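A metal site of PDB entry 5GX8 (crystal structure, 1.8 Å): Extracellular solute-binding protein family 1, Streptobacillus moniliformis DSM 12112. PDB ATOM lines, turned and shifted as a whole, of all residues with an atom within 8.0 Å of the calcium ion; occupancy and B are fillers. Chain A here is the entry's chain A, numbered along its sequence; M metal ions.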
ATOM      1  N   TRP A 137      -8.822  14.825  12.697  1.00  0.00           N
ATOM      2  CA  TRP A 137      -8.999  13.388  12.915  1.00  0.00           C
ATOM      3  C   TRP A 137      -9.999  12.790  11.940  1.00  0.00           C
ATOM      4  O   TRP A 137      -9.758  11.690  11.412  1.00  0.00           O
ATOM      5  CB  TRP A 137      -9.412  13.113  14.361  1.00  0.00           C
ATOM      6  CG  TRP A 137      -8.266  13.331  15.332  1.00  0.00           C
ATOM      7  CD1 TRP A 137      -7.025  13.822  15.038  1.00  0.00           C
ATOM      8  CD2 TRP A 137      -8.253  12.998  16.727  1.00  0.00           C
ATOM      9  NE1 TRP A 137      -6.211  13.818  16.187  1.00  0.00           N
ATOM     10  CE2 TRP A 137      -6.947  13.322  17.225  1.00  0.00           C
ATOM     11  CE3 TRP A 137      -9.205  12.492  17.609  1.00  0.00           C
ATOM     12  CZ2 TRP A 137      -6.590  13.140  18.573  1.00  0.00           C
ATOM     13  CZ3 TRP A 137      -8.836  12.303  18.983  1.00  0.00           C
ATOM     14  CH2 TRP A 137      -7.533  12.623  19.417  1.00  0.00           C
ATOM     15  N   PHE A 159     -12.361   7.008  16.392  1.00  0.00           N
ATOM     16  CA  PHE A 159     -11.379   7.746  17.182  1.00  0.00           C
ATOM     17  C   PHE A 159     -10.728   6.852  18.232  1.00  0.00           C
ATOM     18  O   PHE A 159      -9.537   6.977  18.514  1.00  0.00           O
ATOM     19  CB  PHE A 159     -12.055   8.910  17.930  1.00  0.00           C
ATOM     20  CG  PHE A 159     -12.437  10.088  17.044  1.00  0.00           C
ATOM     21  CD1 PHE A 159     -12.177  10.092  15.683  1.00  0.00           C
ATOM     22  CD2 PHE A 159     -13.003  11.222  17.623  1.00  0.00           C
ATOM     23  CE1 PHE A 159     -12.550  11.214  14.879  1.00  0.00           C
ATOM     24  CE2 PHE A 159     -13.359  12.322  16.862  1.00  0.00           C
ATOM     25  CZ  PHE A 159     -13.119  12.305  15.470  1.00  0.00           C
ATOM     26  N   ARG A 160     -11.528   5.999  18.867  1.00  0.00           N
ATOM     27  CA  ARG A 160     -11.013   5.210  19.982  1.00  0.00           C
ATOM     28  C   ARG A 160     -10.119   4.075  19.492  1.00  0.00           C
ATOM     29  O   ARG A 160      -9.125   3.759  20.155  1.00  0.00           O
ATOM     30  CB  ARG A 160     -12.163   4.657  20.829  1.00  0.00           C
ATOM     31  CG  ARG A 160     -11.726   3.745  21.993  1.00  0.00           C
ATOM     32  CD  ARG A 160     -10.857   4.506  23.027  1.00  0.00           C
ATOM     33  NE  ARG A 160     -10.440   3.621  24.136  1.00  0.00           N
ATOM     34  CZ  ARG A 160      -9.562   3.926  25.103  1.00  0.00           C
ATOM     35  NH1 ARG A 160      -8.919   5.099  25.149  1.00  0.00           N
ATOM     36  NH2 ARG A 160      -9.300   3.004  26.035  1.00  0.00           N
ATOM     37  N   GLU A 161     -10.446   3.490  18.333  1.00  0.00           N
ATOM     38  CA  GLU A 161      -9.796   2.278  17.872  1.00  0.00           C
ATOM     39  C   GLU A 161      -8.698   2.517  16.857  1.00  0.00           C
ATOM     40  O   GLU A 161      -7.839   1.638  16.691  1.00  0.00           O
ATOM     41  CB  GLU A 161     -10.830   1.319  17.262  1.00  0.00           C
ATOM     42  CG  GLU A 161     -11.908   0.867  18.247  1.00  0.00           C
ATOM     43  CD  GLU A 161     -12.912  -0.109  17.650  1.00  0.00           C
ATOM     44  OE1 GLU A 161     -13.384  -0.992  18.415  1.00  0.00           O
ATOM     45  OE2 GLU A 161     -13.253  -0.007  16.436  1.00  0.00           O
ATOM     46  N   LYS A 162      -8.647   3.682  16.197  1.00  0.00           N
ATOM     47  CA  LYS A 162      -7.786   3.818  15.027  1.00  0.00           C
ATOM     48  C   LYS A 162      -6.634   4.797  15.232  1.00  0.00           C
ATOM     49  O   LYS A 162      -6.043   5.259  14.244  1.00  0.00           O
ATOM     50  CB  LYS A 162      -8.605   4.184  13.792  1.00  0.00           C
ATOM     51  CG  LYS A 162      -9.806   3.262  13.581  1.00  0.00           C
ATOM     52  CD  LYS A 162      -9.936   2.719  12.126  1.00  0.00           C
ATOM     53  CE  LYS A 162      -8.809   1.741  11.786  1.00  0.00           C
ATOM     54  NZ  LYS A 162      -9.024   0.899  10.558  1.00  0.00           N
ATOM     55  N   ASP A 163      -6.287   5.102  16.488  1.00  0.00           N
ATOM     56  CA  ASP A 163      -5.070   5.835  16.823  1.00  0.00           C
ATOM     57  C   ASP A 163      -4.849   7.115  16.019  1.00  0.00           C
ATOM     58  O   ASP A 163      -3.762   7.330  15.480  1.00  0.00           O
ATOM     59  CB  ASP A 163      -3.885   4.892  16.646  1.00  0.00           C
ATOM     60  CG  ASP A 163      -2.596   5.464  17.195  1.00  0.00           C
ATOM     61  OD1 ASP A 163      -2.634   6.177  18.218  1.00  0.00           O
ATOM     62  OD2 ASP A 163      -1.527   5.147  16.583  1.00  0.00           O
ATOM     63  N   PRO A 164      -5.854   7.997  15.925  1.00  0.00           N
ATOM     64  CA  PRO A 164      -5.627   9.250  15.196  1.00  0.00           C
ATOM     65  C   PRO A 164      -4.535  10.139  15.797  1.00  0.00           C
ATOM     66  O   PRO A 164      -4.014  10.981  15.077  1.00  0.00           O
ATOM     67  CB  PRO A 164      -6.999   9.960  15.267  1.00  0.00           C
ATOM     68  CG  PRO A 164      -7.576   9.478  16.564  1.00  0.00           C
ATOM     69  CD  PRO A 164      -7.159   8.005  16.625  1.00  0.00           C
ATOM     70  N   ASN A 165      -4.184  10.048  17.085  1.00  0.00           N
ATOM     71  CA  ASN A 165      -3.073  10.921  17.450  1.00  0.00           C
ATOM     72  C   ASN A 165      -1.711  10.312  17.057  1.00  0.00           C
ATOM     73  O   ASN A 165      -0.696  11.001  17.164  1.00  0.00           O
ATOM     74  CB  ASN A 165      -3.102  11.347  18.943  1.00  0.00           C
ATOM     75  CG  ASN A 165      -2.956  10.196  19.936  1.00  0.00           C
ATOM     76  OD1 ASN A 165      -2.405   9.131  19.632  1.00  0.00           O
ATOM     77  ND2 ASN A 165      -3.445  10.433  21.139  1.00  0.00           N
ATOM     78  N   GLY A 166      -1.711   9.086  16.550  1.00  0.00           N
ATOM     79  CA  GLY A 166      -0.551   8.560  15.839  1.00  0.00           C
ATOM     80  C   GLY A 166       0.534   8.021  16.718  1.00  0.00           C
ATOM     81  O   GLY A 166       1.671   7.832  16.256  1.00  0.00           O
ATOM     82  N   ASN A 167       0.260   7.749  17.983  1.00  0.00           N
ATOM     83  CA  ASN A 167       1.331   7.347  18.872  1.00  0.00           C
ATOM     84  C   ASN A 167       1.363   5.846  19.127  1.00  0.00           C
ATOM     85  O   ASN A 167       2.109   5.403  19.993  1.00  0.00           O
ATOM     86  CB  ASN A 167       1.273   8.135  20.189  1.00  0.00           C
ATOM     87  CG  ASN A 167      -0.005   7.888  21.012  1.00  0.00           C
ATOM     88  OD1 ASN A 167      -0.839   7.038  20.676  1.00  0.00           O
ATOM     89  ND2 ASN A 167      -0.123   8.610  22.120  1.00  0.00           N
ATOM     90  N   GLY A 168       0.606   5.058  18.363  1.00  0.00           N
ATOM     91  CA  GLY A 168       0.546   3.609  18.592  1.00  0.00           C
ATOM     92  C   GLY A 168       0.011   3.192  19.943  1.00  0.00           C
ATOM     93  O   GLY A 168       0.300   2.079  20.403  1.00  0.00           O
ATOM     94  N   LYS A 169      -0.745   4.061  20.608  1.00  0.00           N
ATOM     95  CA  LYS A 169      -1.350   3.792  21.910  1.00  0.00           C
ATOM     96  C   LYS A 169      -2.856   4.037  21.829  1.00  0.00           C
ATOM     97  O   LYS A 169      -3.304   4.967  21.160  1.00  0.00           O
ATOM     98  CB  LYS A 169      -0.747   4.664  23.030  1.00  0.00           C
ATOM     99  CG  LYS A 169       0.761   4.478  23.255  1.00  0.00           C
ATOM    100  CD  LYS A 169       1.234   5.492  24.291  1.00  0.00           C
ATOM    101  CE  LYS A 169       2.745   5.465  24.470  1.00  0.00           C
ATOM    102  NZ  LYS A 169       3.196   6.660  25.255  1.00  0.00           N
ATOM    103  N   LYS A 170      -3.620   3.174  22.486  1.00  0.00           N
ATOM    104  CA  LYS A 170      -5.070   3.367  22.562  1.00  0.00           C
ATOM    105  C   LYS A 170      -5.349   4.287  23.733  1.00  0.00           C
ATOM    106  O   LYS A 170      -5.712   3.863  24.839  1.00  0.00           O
ATOM    107  CB  LYS A 170      -5.765   2.022  22.671  1.00  0.00           C
ATOM    108  CG  LYS A 170      -7.283   2.064  22.593  1.00  0.00           C
ATOM    109  CD  LYS A 170      -7.841   0.642  22.618  1.00  0.00           C
ATOM    110  CE  LYS A 170      -9.311   0.628  22.204  1.00  0.00           C
ATOM    111  NZ  LYS A 170      -9.878  -0.750  22.087  1.00  0.00           N
ATOM    112  N   ASP A 171      -5.093   5.587  23.521  1.00  0.00           N
ATOM    113  CA  ASP A 171      -5.208   6.560  24.577  1.00  0.00           C
ATOM    114  C   ASP A 171      -6.236   7.639  24.270  1.00  0.00           C
ATOM    115  O   ASP A 171      -6.471   8.509  25.124  1.00  0.00           O
ATOM    116  CB  ASP A 171      -3.841   7.204  24.867  1.00  0.00           C
ATOM    117  CG  ASP A 171      -3.234   7.813  23.648  1.00  0.00           C
ATOM    118  OD1 ASP A 171      -3.717   7.524  22.557  1.00  0.00           O
ATOM    119  OD2 ASP A 171      -2.267   8.589  23.792  1.00  0.00           O
ATOM    120  N   GLU A 172      -6.827   7.583  23.096  1.00  0.00           N
ATOM    121  CA  GLU A 172      -7.755   8.607  22.626  1.00  0.00           C
ATOM    122  C   GLU A 172      -8.986   8.634  23.520  1.00  0.00           C
ATOM    123  O   GLU A 172      -9.489   7.586  23.941  1.00  0.00           O
ATOM    124  CB  GLU A 172      -8.146   8.340  21.166  1.00  0.00           C
ATOM    125  CG  GLU A 172      -7.119   8.842  20.101  1.00  0.00           C
ATOM    126  CD  GLU A 172      -5.937   7.886  19.895  1.00  0.00           C
ATOM    127  OE1 GLU A 172      -5.942   6.814  20.529  1.00  0.00           O
ATOM    128  OE2 GLU A 172      -5.031   8.220  19.106  1.00  0.00           O
ATOM    129  N   VAL A 173      -9.460   9.842  23.800  1.00  0.00           N
ATOM    130  CA  VAL A 173     -10.662  10.081  24.574  1.00  0.00           C
ATOM    131  C   VAL A 173     -11.677  10.698  23.604  1.00  0.00           C
ATOM    132  O   VAL A 173     -11.656  11.921  23.443  1.00  0.00           O
ATOM    133  CB  VAL A 173     -10.360  11.001  25.779  1.00  0.00           C
ATOM    134  CG1 VAL A 173     -11.628  11.348  26.548  1.00  0.00           C
ATOM    135  CG2 VAL A 173      -9.299  10.281  26.790  1.00  0.00           C
ATOM    136  N   ASN A 250      -3.449  16.195  23.086  1.00  0.00           N
ATOM    137  CA  ASN A 250      -3.879  15.563  21.841  1.00  0.00           C
ATOM    138  C   ASN A 250      -4.566  14.220  22.091  1.00  0.00           C
ATOM    139  O   ASN A 250      -4.387  13.243  21.329  1.00  0.00           O
ATOM    140  CB  ASN A 250      -2.696  15.400  20.869  1.00  0.00           C
ATOM    141  CG  ASN A 250      -3.173  15.315  19.464  1.00  0.00           C
ATOM    142  OD1 ASN A 250      -4.307  15.734  19.154  1.00  0.00           O
ATOM    143  ND2 ASN A 250      -2.334  14.748  18.581  1.00  0.00           N
ATOM    144  N   LEU A 251      -5.414  14.173  23.120  1.00  0.00           N
ATOM    145  CA  LEU A 251      -6.204  13.000  23.445  1.00  0.00           C
ATOM    146  C   LEU A 251      -7.678  13.160  23.118  1.00  0.00           C
ATOM    147  O   LEU A 251      -8.326  12.162  22.784  1.00  0.00           O
ATOM    148  CB  LEU A 251      -6.084  12.702  24.951  1.00  0.00           C
ATOM    149  CG  LEU A 251      -4.680  12.453  25.544  1.00  0.00           C
ATOM    150  CD1 LEU A 251      -4.815  12.362  27.100  1.00  0.00           C
ATOM    151  CD2 LEU A 251      -4.072  11.166  24.976  1.00  0.00           C
HETATM  152 CA    CA M   1      -3.290   7.117  20.191  1.00  0.00          CA
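The side-chain amide nitrogen (ND2) of Asn 165 is in hydrogen-bond range of the backbone carbonyl oxygen (O) of Asn 250 (3.0 Å).
OD1 of Asp 163 sits close to N of Gly 166 (3.5 Å).
The side-chain carboxylate (OD2) of Asp 163 is in hydrogen-bond range of the backbone NH (N) of Gly 168.
O of Glu 172 sits at hydrogen-bond distance from NH1 of Arg 160 (2.8 Å).
Six residues have an atom within 4 Å of the calcium ion: Asp 163, Asn 165, Asn 167, Lys 169, Asp 171 and Glu 172.
The side-chain amide oxygen (OD1) of Asn 165 is bound to the calcium ion (2.3 Å).
The calcium ion is bound by OD1 of Asp 163, at 2.3 Å.
OE2 of Glu 172 is bound to the calcium ion (2.3 Å).
The backbone carbonyl oxygen (O) of Lys 169 is bound to the calcium ion (2.4 Å).
OD1 of Asp 171 is bound to the calcium ion, at 2.4 Å.
OD1 of Asn 167 binds the calcium ion, 2.5 Å away.
The calcium ion is bound by OE1 of Glu 172 (2.7 Å).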
